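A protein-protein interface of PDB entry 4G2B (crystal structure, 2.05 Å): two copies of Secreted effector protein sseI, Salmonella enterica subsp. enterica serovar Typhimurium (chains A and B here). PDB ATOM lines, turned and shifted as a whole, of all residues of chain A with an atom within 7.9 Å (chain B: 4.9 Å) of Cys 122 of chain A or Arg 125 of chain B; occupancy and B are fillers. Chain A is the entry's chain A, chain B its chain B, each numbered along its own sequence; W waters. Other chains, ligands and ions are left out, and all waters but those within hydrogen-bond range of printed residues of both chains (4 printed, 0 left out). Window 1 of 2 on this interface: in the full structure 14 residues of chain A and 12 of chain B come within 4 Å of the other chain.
The backbone carbonyl oxygen (O) of Met 126 of chain B lies within hydrogen-bond range of the side-chain hydroxyl (OG1) of Thr 9 of chain A (3.4 Å). SG of Cys 122 of chain A forms a disulfide with SG of Cys 122 of chain B (2.2 Å). NH1 of Arg 125 of chain B is in hydrogen-bond range of SG of Cys 122 of chain A (3.5 Å). OH of Tyr 10 of chain A is in hydrogen-bond range of O of Arg 125 of chain B (3.5 Å).
NZ of Lys 123 of chain A sits at hydrogen-bond distance from O of Tyr 10 of chain A (3.1 Å). The backbone NH (N) of Ser 116 of chain A sits at hydrogen-bond distance from the side-chain carboxylate (OE1) of Glu 119 of chain A (2.7 Å). NH2 of Arg 125 of chain A lies close to O of Val 166 of chain A, at 3.4 Å. The side-chain hydroxyl (OH) of Tyr 10 of chain A lies within hydrogen-bond range of the side-chain carboxylate (OE2) of Glu 119 of chain A (2.9 Å). The backbone carbonyl oxygen (O) of Thr 9 of chain A sits at hydrogen-bond distance from the side-chain amino group (NZ) of Lys 123 of chain A, at 2.8 Å.
Among the printed residues, merely in contact across the chains: Tyr 10 of chain A with Met 126 of chain B (2.8 Å), Cys 122 of chain A with Met 126 of chain B (3.5 Å), Glu 119 of chain A with Met 126 of chain B (3.5 Å), Tyr 10 of chain A with Thr 128 of chain B (3.6 Å), Arg 125 of chain A with Cys 122 of chain B (3.7 Å), Met 126 of chain A with Cys 122 of chain B (3.7 Å) and Asp 118 of chain A with Arg 125 of chain B (3.999 Å).
Of the printed residues of chain B, Thr 9 of chain A touches Met 126 (3.4 Å). Of the printed residues of chain B, Arg 125 of chain A touches Cys 122. Of the printed residues of chain B, Met 126 of chain A touches Cys 122. Of the printed residues of chain A, Arg 125 of chain B touches Tyr 10, Asp 118 and Cys 122. Of the printed residues of chain A, Met 126 of chain B touches Thr 9, Tyr 10, Glu 119 and Cys 122. Printed residues of chain A within 4 Å of Thr 128 of chain B: Tyr 10. The nearest printed residue of chain B that does not touch Cys 122 of chain A is Val 121 of chain B (5.0 Å). The nearest printed residue of chain A that does not touch Arg 125 of chain B is Glu 119 of chain A (4.3 Å).
Of the 10 printed residues of chain B, 4 touch a printed residue of chain A. Printed residues of chain B that touch a printed residue of chain A: Cys 122, Arg 125, Met 126 and Thr 128.
Cys 122 of chain B touches its own counterpart, Cys 122 of chain A. Cys 122 of chain A touches Arg 125 of chain B, and with the chains exchanged Arg 125 of chain A touches Cys 122 of chain B. Cys 122 of chain A touches Met 126 of chain B, and with the chains exchanged Met 126 of chain A touches Cys 122 of chain B. Of the 11 pairs that touch across the chains among the printed residues, 5 have their exchanged pair printed and touching as well.
Water W3 lies within hydrogen-bond range of the guanidinium group of Arg 125 of chain A and the side-chain sulfur of Cys 122 of chain B. Water W1 lies within hydrogen-bond range of O of Arg 125 of chain B (2.7 Å), OH of Tyr 10 of chain A (2.7 Å) and O of Thr 128 of chain B (2.8 Å). Water W2 lies within hydrogen-bond range of the backbone carbonyl oxygen (O) of Lys 123 of chain B and the side-chain hydroxyl (OG1) of Thr 9 of chain A. Water W4 lies within hydrogen-bond range of O of Asp 118 of chain A (2.9 Å), NH1 of Arg 125 of chain B (3.5 Å) and SG of Cys 122 of chain A (3.7 Å).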
ATOM      1  N   THR A   9      22.831  16.261 -19.635  1.00  0.00           N
ATOM      2  CA  THR A   9      23.360  16.799 -18.330  1.00  0.00           C
ATOM      3  C   THR A   9      22.930  18.295 -18.241  1.00  0.00           C
ATOM      4  O   THR A   9      22.934  18.992 -19.232  1.00  0.00           O
ATOM      5  CB  THR A   9      24.877  16.423 -18.319  1.00  0.00           C
ATOM      6  OG1 THR A   9      25.075  15.216 -17.525  1.00  0.00           O
ATOM      7  CG2 THR A   9      25.801  17.524 -17.911  1.00  0.00           C
ATOM      8  N   TYR A  10      22.498  18.787 -17.080  1.00  0.00           N
ATOM      9  CA  TYR A  10      21.886  20.110 -17.054  1.00  0.00           C
ATOM     10  C   TYR A  10      22.888  21.277 -17.266  1.00  0.00           C
ATOM     11  O   TYR A  10      24.050  21.167 -16.941  1.00  0.00           O
ATOM     12  CB  TYR A  10      21.165  20.332 -15.776  1.00  0.00           C
ATOM     13  CG  TYR A  10      21.939  20.222 -14.485  1.00  0.00           C
ATOM     14  CD1 TYR A  10      21.979  19.004 -13.769  1.00  0.00           C
ATOM     15  CD2 TYR A  10      22.467  21.353 -13.891  1.00  0.00           C
ATOM     16  CE1 TYR A  10      22.578  18.935 -12.571  1.00  0.00           C
ATOM     17  CE2 TYR A  10      23.062  21.306 -12.693  1.00  0.00           C
ATOM     18  CZ  TYR A  10      23.124  20.081 -12.029  1.00  0.00           C
ATOM     19  OH  TYR A  10      23.681  20.015 -10.821  1.00  0.00           O
ATOM     20  N   ASN A 108      28.919  17.352 -25.180  1.00  0.00           N
ATOM     21  CA  ASN A 108      28.201  17.569 -23.955  1.00  0.00           C
ATOM     22  C   ASN A 108      28.011  19.066 -23.612  1.00  0.00           C
ATOM     23  O   ASN A 108      27.127  19.404 -22.880  1.00  0.00           O
ATOM     24  CB  ASN A 108      28.842  16.765 -22.834  1.00  0.00           C
ATOM     25  CG  ASN A 108      28.934  15.259 -23.191  1.00  0.00           C
ATOM     26  OD1 ASN A 108      28.274  14.792 -24.150  1.00  0.00           O
ATOM     27  ND2 ASN A 108      29.764  14.496 -22.439  1.00  0.00           N
ATOM     28  N   LEU A 109      28.788  19.958 -24.214  1.00  0.00           N
ATOM     29  CA  LEU A 109      28.602  21.387 -24.017  1.00  0.00           C
ATOM     30  C   LEU A 109      27.658  21.944 -25.077  1.00  0.00           C
ATOM     31  O   LEU A 109      28.092  22.522 -26.035  1.00  0.00           O
ATOM     32  CB  LEU A 109      29.969  22.114 -24.063  1.00  0.00           C
ATOM     33  CG  LEU A 109      30.996  21.810 -22.951  1.00  0.00           C
ATOM     34  CD1 LEU A 109      32.178  22.772 -23.110  1.00  0.00           C
ATOM     35  CD2 LEU A 109      30.409  21.959 -21.562  1.00  0.00           C
ATOM     36  N   LEU A 115      26.057  27.976 -13.883  1.00  0.00           N
ATOM     37  CA  LEU A 115      26.192  26.906 -12.929  1.00  0.00           C
ATOM     38  C   LEU A 115      26.919  27.313 -11.701  1.00  0.00           C
ATOM     39  O   LEU A 115      27.622  28.343 -11.709  1.00  0.00           O
ATOM     40  CB  LEU A 115      26.985  25.768 -13.573  1.00  0.00           C
ATOM     41  CG  LEU A 115      26.324  25.053 -14.741  1.00  0.00           C
ATOM     42  CD1 LEU A 115      27.336  24.234 -15.478  1.00  0.00           C
ATOM     43  CD2 LEU A 115      25.207  24.132 -14.214  1.00  0.00           C
ATOM     44  N   SER A 116      26.825  26.463 -10.663  1.00  0.00           N
ATOM     45  CA  SER A 116      27.608  26.645  -9.459  1.00  0.00           C
ATOM     46  C   SER A 116      29.072  26.452  -9.854  1.00  0.00           C
ATOM     47  O   SER A 116      29.329  25.834 -10.856  1.00  0.00           O
ATOM     48  CB  SER A 116      27.146  25.670  -8.357  1.00  0.00           C
ATOM     49  OG  SER A 116      27.708  24.414  -8.610  1.00  0.00           O
ATOM     50  N   ALA A 117      30.034  26.954  -9.088  1.00  0.00           N
ATOM     51  CA  ALA A 117      31.469  26.696  -9.445  1.00  0.00           C
ATOM     52  C   ALA A 117      31.732  25.200  -9.632  1.00  0.00           C
ATOM     53  O   ALA A 117      32.410  24.765 -10.556  1.00  0.00           O
ATOM     54  CB  ALA A 117      32.477  27.282  -8.304  1.00  0.00           C
ATOM     55  N   ASP A 118      31.214  24.396  -8.724  1.00  0.00           N
ATOM     56  CA  ASP A 118      31.538  22.975  -8.799  1.00  0.00           C
ATOM     57  C   ASP A 118      30.822  22.311  -9.953  1.00  0.00           C
ATOM     58  O   ASP A 118      31.404  21.444 -10.640  1.00  0.00           O
ATOM     59  CB  ASP A 118      31.132  22.297  -7.507  1.00  0.00           C
ATOM     60  CG  ASP A 118      32.211  22.388  -6.428  1.00  0.00           C
ATOM     61  OD1 ASP A 118      33.404  22.562  -6.784  1.00  0.00           O
ATOM     62  OD2 ASP A 118      31.865  22.227  -5.235  1.00  0.00           O
ATOM     63  N   GLU A 119      29.587  22.682 -10.176  1.00  0.00           N
ATOM     64  CA  GLU A 119      28.857  22.196 -11.344  1.00  0.00           C
ATOM     65  C   GLU A 119      29.577  22.554 -12.634  1.00  0.00           C
ATOM     66  O   GLU A 119      29.601  21.761 -13.550  1.00  0.00           O
ATOM     67  CB  GLU A 119      27.427  22.748 -11.381  1.00  0.00           C
ATOM     68  CG  GLU A 119      26.490  22.078 -10.415  1.00  0.00           C
ATOM     69  CD  GLU A 119      25.333  22.985 -10.069  1.00  0.00           C
ATOM     70  OE1 GLU A 119      25.364  24.163 -10.454  1.00  0.00           O
ATOM     71  OE2 GLU A 119      24.358  22.538  -9.471  1.00  0.00           O
ATOM     72  N   TRP A 120      30.167  23.753 -12.713  1.00  0.00           N
ATOM     73  CA  TRP A 120      30.783  24.209 -13.919  1.00  0.00           C
ATOM     74  C   TRP A 120      32.022  23.304 -14.162  1.00  0.00           C
ATOM     75  O   TRP A 120      32.230  22.795 -15.291  1.00  0.00           O
ATOM     76  CB  TRP A 120      31.161  25.731 -13.837  1.00  0.00           C
ATOM     77  CG  TRP A 120      31.773  26.223 -15.040  1.00  0.00           C
ATOM     78  CD1 TRP A 120      31.146  26.721 -16.125  1.00  0.00           C
ATOM     79  CD2 TRP A 120      33.171  26.245 -15.331  1.00  0.00           C
ATOM     80  NE1 TRP A 120      32.061  27.019 -17.092  1.00  0.00           N
ATOM     81  CE2 TRP A 120      33.317  26.767 -16.616  1.00  0.00           C
ATOM     82  CE3 TRP A 120      34.308  25.806 -14.646  1.00  0.00           C
ATOM     83  CZ2 TRP A 120      34.589  26.870 -17.270  1.00  0.00           C
ATOM     84  CZ3 TRP A 120      35.550  25.953 -15.260  1.00  0.00           C
ATOM     85  CH2 TRP A 120      35.673  26.504 -16.537  1.00  0.00           C
ATOM     86  N   VAL A 121      32.764  23.042 -13.093  1.00  0.00           N
ATOM     87  CA  VAL A 121      33.931  22.152 -13.190  1.00  0.00           C
ATOM     88  C   VAL A 121      33.512  20.800 -13.716  1.00  0.00           C
ATOM     89  O   VAL A 121      34.185  20.286 -14.582  1.00  0.00           O
ATOM     90  CB  VAL A 121      34.722  22.079 -11.898  1.00  0.00           C
ATOM     91  CG1 VAL A 121      35.758  20.965 -11.892  1.00  0.00           C
ATOM     92  CG2 VAL A 121      35.417  23.454 -11.683  1.00  0.00           C
ATOM     93  N   CYS A 122      32.439  20.232 -13.164  1.00  0.00           N
ATOM     94  CA  CYS A 122      32.002  18.863 -13.560  1.00  0.00           C
ATOM     95  C   CYS A 122      31.648  18.829 -15.031  1.00  0.00           C
ATOM     96  O   CYS A 122      32.014  17.905 -15.735  1.00  0.00           O
ATOM     97  CB  CYS A 122      30.815  18.376 -12.714  1.00  0.00           C
ATOM     98  SG  CYS A 122      31.341  17.911 -11.105  1.00  0.00           S
ATOM     99  N   LYS A 123      30.954  19.872 -15.490  1.00  0.00           N
ATOM    100  CA  LYS A 123      30.515  19.972 -16.857  1.00  0.00           C
ATOM    101  C   LYS A 123      31.696  19.898 -17.812  1.00  0.00           C
ATOM    102  O   LYS A 123      31.697  19.122 -18.796  1.00  0.00           O
ATOM    103  CB  LYS A 123      29.727  21.255 -17.091  1.00  0.00           C
ATOM    104  CG  LYS A 123      28.932  21.303 -18.343  1.00  0.00           C
ATOM    105  CD  LYS A 123      27.609  20.538 -18.249  1.00  0.00           C
ATOM    106  CE  LYS A 123      26.929  20.388 -19.549  1.00  0.00           C
ATOM    107  NZ  LYS A 123      25.536  19.885 -19.367  1.00  0.00           N
ATOM    108  N   TYR A 124      32.712  20.683 -17.535  1.00  0.00           N
ATOM    109  CA  TYR A 124      33.890  20.647 -18.348  1.00  0.00           C
ATOM    110  C   TYR A 124      34.674  19.358 -18.184  1.00  0.00           C
ATOM    111  O   TYR A 124      35.137  18.834 -19.167  1.00  0.00           O
ATOM    112  CB  TYR A 124      34.814  21.888 -18.112  1.00  0.00           C
ATOM    113  CG  TYR A 124      34.390  23.073 -18.952  1.00  0.00           C
ATOM    114  CD1 TYR A 124      33.292  23.825 -18.599  1.00  0.00           C
ATOM    115  CD2 TYR A 124      34.994  23.350 -20.168  1.00  0.00           C
ATOM    116  CE1 TYR A 124      32.853  24.819 -19.408  1.00  0.00           C
ATOM    117  CE2 TYR A 124      34.562  24.361 -20.965  1.00  0.00           C
ATOM    118  CZ  TYR A 124      33.499  25.107 -20.557  1.00  0.00           C
ATOM    119  OH  TYR A 124      33.062  26.155 -21.326  1.00  0.00           O
ATOM    120  N   ARG A 125      34.811  18.868 -16.953  1.00  0.00           N
ATOM    121  CA  ARG A 125      35.631  17.698 -16.668  1.00  0.00           C
ATOM    122  C   ARG A 125      35.069  16.498 -17.436  1.00  0.00           C
ATOM    123  O   ARG A 125      35.798  15.709 -18.089  1.00  0.00           O
ATOM    124  CB  ARG A 125      35.620  17.446 -15.151  1.00  0.00           C
ATOM    125  CG  ARG A 125      36.267  16.191 -14.576  1.00  0.00           C
ATOM    126  CD  ARG A 125      36.127  16.221 -13.039  1.00  0.00           C
ATOM    127  NE  ARG A 125      37.472  16.298 -12.613  1.00  0.00           N
ATOM    128  CZ  ARG A 125      38.004  16.993 -11.651  1.00  0.00           C
ATOM    129  NH1 ARG A 125      37.335  17.769 -10.843  1.00  0.00           N
ATOM    130  NH2 ARG A 125      39.292  16.817 -11.512  1.00  0.00           N
ATOM    131  N   MET A 126      33.756  16.379 -17.388  1.00  0.00           N
ATOM    132  CA  MET A 126      33.159  15.185 -17.932  1.00  0.00           C
ATOM    133  C   MET A 126      32.855  15.292 -19.453  1.00  0.00           C
ATOM    134  O   MET A 126      32.289  14.379 -20.012  1.00  0.00           O
ATOM    135  CB  MET A 126      31.883  14.879 -17.158  1.00  0.00           C
ATOM    136  CG  MET A 126      32.055  14.496 -15.759  1.00  0.00           C
ATOM    137  SD  MET A 126      33.403  13.423 -15.345  1.00  0.00           S
ATOM    138  CE  MET A 126      32.735  11.806 -15.917  1.00  0.00           C
ATOM    139  N   ALA A 127      33.215  16.406 -20.091  1.00  0.00           N
ATOM    140  CA  ALA A 127      32.931  16.674 -21.472  1.00  0.00           C
ATOM    141  C   ALA A 127      34.103  16.199 -22.326  1.00  0.00           C
ATOM    142  O   ALA A 127      33.953  16.082 -23.523  1.00  0.00           O
ATOM    143  CB  ALA A 127      32.684  18.152 -21.722  1.00  0.00           C
ATOM    144  N   THR A 128      35.239  15.897 -21.729  1.00  0.00           N
ATOM    145  CA  THR A 128      36.373  15.406 -22.480  1.00  0.00           C
ATOM    146  C   THR A 128      37.099  14.325 -21.702  1.00  0.00           C
ATOM    147  O   THR A 128      37.207  14.357 -20.487  1.00  0.00           O
ATOM    148  CB  THR A 128      37.349  16.550 -22.934  1.00  0.00           C
ATOM    149  OG1 THR A 128      38.493  15.987 -23.603  1.00  0.00           O
ATOM    150  CG2 THR A 128      37.799  17.396 -21.753  1.00  0.00           C
ATOM    151  N   VAL A 166      40.893  21.685 -14.252  1.00  0.00           N
ATOM    152  CA  VAL A 166      39.619  21.025 -14.418  1.00  0.00           C
ATOM    153  C   VAL A 166      39.877  19.581 -14.793  1.00  0.00           C
ATOM    154  O   VAL A 166      39.155  18.716 -14.323  1.00  0.00           O
ATOM    155  CB  VAL A 166      38.756  21.692 -15.529  1.00  0.00           C
ATOM    156  CG1 VAL A 166      37.456  20.830 -15.867  1.00  0.00           C
ATOM    157  CG2 VAL A 166      38.375  23.084 -15.044  1.00  0.00           C
ATOM    158  N   THR A 167      40.857  19.350 -15.660  1.00  0.00           N
ATOM    159  CA  THR A 167      41.315  17.984 -15.977  1.00  0.00           C
ATOM    160  C   THR A 167      42.791  17.905 -15.783  1.00  0.00           C
ATOM    161  O   THR A 167      43.443  18.920 -15.616  1.00  0.00           O
ATOM    162  CB  THR A 167      40.986  17.548 -17.366  1.00  0.00           C
ATOM    163  OG1 THR A 167      41.786  18.262 -18.326  1.00  0.00           O
ATOM    164  CG2 THR A 167      39.509  17.753 -17.644  1.00  0.00           C
ATOM    165  N   VAL B 121      31.915  11.601  -8.611  1.00  0.00           N
ATOM    166  CA  VAL B 121      31.052  12.560  -7.977  1.00  0.00           C
ATOM    167  C   VAL B 121      30.376  13.424  -9.059  1.00  0.00           C
ATOM    168  O   VAL B 121      29.172  13.736  -8.976  1.00  0.00           O
ATOM    169  CB  VAL B 121      31.841  13.393  -6.928  1.00  0.00           C
ATOM    170  CG1 VAL B 121      31.147  14.688  -6.700  1.00  0.00           C
ATOM    171  CG2 VAL B 121      32.061  12.544  -5.598  1.00  0.00           C
ATOM    172  N   CYS B 122      31.152  13.836 -10.066  1.00  0.00           N
ATOM    173  CA  CYS B 122      30.602  14.679 -11.133  1.00  0.00           C
ATOM    174  C   CYS B 122      29.518  13.958 -11.922  1.00  0.00           C
ATOM    175  O   CYS B 122      28.493  14.539 -12.318  1.00  0.00           O
ATOM    176  CB  CYS B 122      31.709  15.033 -12.137  1.00  0.00           C
ATOM    177  SG  CYS B 122      32.778  16.346 -11.541  1.00  0.00           S
ATOM    178  N   LYS B 123      29.772  12.673 -12.185  1.00  0.00           N
ATOM    179  CA  LYS B 123      28.801  11.862 -12.882  1.00  0.00           C
ATOM    180  C   LYS B 123      27.438  11.867 -12.147  1.00  0.00           C
ATOM    181  O   LYS B 123      26.414  12.140 -12.749  1.00  0.00           O
ATOM    182  CB  LYS B 123      29.362  10.437 -13.022  1.00  0.00           C
ATOM    183  CG  LYS B 123      28.663   9.598 -14.080  1.00  0.00           C
ATOM    184  CD  LYS B 123      29.087   9.896 -15.515  1.00  0.00           C
ATOM    185  CE  LYS B 123      28.086   9.275 -16.506  1.00  0.00           C
ATOM    186  NZ  LYS B 123      28.457   9.499 -17.974  1.00  0.00           N
ATOM    187  N   TYR B 124      27.423  11.548 -10.851  1.00  0.00           N
ATOM    188  CA  TYR B 124      26.166  11.611 -10.081  1.00  0.00           C
ATOM    189  C   TYR B 124      25.591  13.030  -9.909  1.00  0.00           C
ATOM    190  O   TYR B 124      24.399  13.212 -10.038  1.00  0.00           O
ATOM    191  CB  TYR B 124      26.327  10.979  -8.732  1.00  0.00           C
ATOM    192  CG  TYR B 124      26.173   9.460  -8.768  1.00  0.00           C
ATOM    193  CD1 TYR B 124      27.167   8.665  -9.321  1.00  0.00           C
ATOM    194  CD2 TYR B 124      25.019   8.832  -8.290  1.00  0.00           C
ATOM    195  CE1 TYR B 124      27.032   7.305  -9.362  1.00  0.00           C
ATOM    196  CE2 TYR B 124      24.872   7.446  -8.350  1.00  0.00           C
ATOM    197  CZ  TYR B 124      25.881   6.698  -8.872  1.00  0.00           C
ATOM    198  OH  TYR B 124      25.789   5.325  -8.883  1.00  0.00           O
ATOM    199  N   ARG B 125      26.442  13.991  -9.568  1.00  0.00           N
ATOM    200  CA  ARG B 125      26.005  15.381  -9.355  1.00  0.00           C
ATOM    201  C   ARG B 125      25.267  15.941 -10.543  1.00  0.00           C
ATOM    202  O   ARG B 125      24.206  16.593 -10.421  1.00  0.00           O
ATOM    203  CB  ARG B 125      27.253  16.245  -9.076  1.00  0.00           C
ATOM    204  CG  ARG B 125      27.025  17.743  -8.887  1.00  0.00           C
ATOM    205  CD  ARG B 125      28.350  18.501  -8.891  1.00  0.00           C
ATOM    206  NE  ARG B 125      28.747  18.675  -7.514  1.00  0.00           N
ATOM    207  CZ  ARG B 125      29.949  18.513  -6.983  1.00  0.00           C
ATOM    208  NH1 ARG B 125      31.085  18.147  -7.662  1.00  0.00           N
ATOM    209  NH2 ARG B 125      30.003  18.708  -5.683  1.00  0.00           N
ATOM    210  N   MET B 126      25.828  15.704 -11.698  1.00  0.00           N
ATOM    211  CA  MET B 126      25.283  16.243 -12.933  1.00  0.00           C
ATOM    212  C   MET B 126      24.154  15.403 -13.536  1.00  0.00           C
ATOM    213  O   MET B 126      23.619  15.810 -14.546  1.00  0.00           O
ATOM    214  CB  MET B 126      26.375  16.443 -13.971  1.00  0.00           C
ATOM    215  CG  MET B 126      27.527  17.363 -13.458  1.00  0.00           C
ATOM    216  SD  MET B 126      26.879  19.003 -12.974  1.00  0.00           S
ATOM    217  CE  MET B 126      26.124  18.712 -11.388  1.00  0.00           C
ATOM    218  N   ALA B 127      23.844  14.245 -12.952  1.00  0.00           N
ATOM    219  CA  ALA B 127      22.770  13.351 -13.451  1.00  0.00           C
ATOM    220  C   ALA B 127      21.413  13.815 -12.934  1.00  0.00           C
ATOM    221  O   ALA B 127      20.356  13.341 -13.350  1.00  0.00           O
ATOM    222  CB  ALA B 127      23.017  11.846 -12.939  1.00  0.00           C
ATOM    223  N   THR B 128      21.435  14.641 -11.916  1.00  0.00           N
ATOM    224  CA  THR B 128      20.195  15.044 -11.274  1.00  0.00           C
ATOM    225  C   THR B 128      20.335  16.403 -10.611  1.00  0.00           C
ATOM    226  O   THR B 128      21.331  16.736 -10.048  1.00  0.00           O
ATOM    227  CB  THR B 128      19.724  14.021 -10.198  1.00  0.00           C
ATOM    228  OG1 THR B 128      18.510  14.486  -9.616  1.00  0.00           O
ATOM    229  CG2 THR B 128      20.739  13.839  -9.063  1.00  0.00           C
ATOM    230  N   VAL B 166      26.994  14.471  -2.326  1.00  0.00           N
ATOM    231  CA  VAL B 166      27.315  14.544  -3.753  1.00  0.00           C
ATOM    232  C   VAL B 166      26.498  15.680  -4.369  1.00  0.00           C
ATOM    233  O   VAL B 166      26.972  16.413  -5.226  1.00  0.00           O
ATOM    234  CB  VAL B 166      27.048  13.189  -4.448  1.00  0.00           C
ATOM    235  CG1 VAL B 166      27.021  13.300  -5.967  1.00  0.00           C
ATOM    236  CG2 VAL B 166      28.112  12.244  -4.070  1.00  0.00           C
ATOM    237  N   THR B 167      25.245  15.776  -3.960  1.00  0.00           N
ATOM    238  CA  THR B 167      24.375  16.922  -4.271  1.00  0.00           C
ATOM    239  C   THR B 167      23.806  17.471  -2.974  1.00  0.00           C
ATOM    240  O   THR B 167      23.904  16.839  -1.893  1.00  0.00           O
ATOM    241  CB  THR B 167      23.204  16.477  -5.136  1.00  0.00           C
ATOM    242  OG1 THR B 167      22.434  15.544  -4.388  1.00  0.00           O
ATOM    243  CG2 THR B 167      23.699  15.802  -6.403  1.00  0.00           C
HETATM  244  O   HOH W   1      23.164  18.405  -8.723  1.00  0.00           O
HETATM  245  O   HOH W   2      26.206  12.682 -15.424  1.00  0.00           O
HETATM  246  O   HOH W   3      35.058  18.076 -10.053  1.00  0.00           O
HETATM  247  O   HOH W   4      33.512  20.145  -9.186  1.00  0.00           O
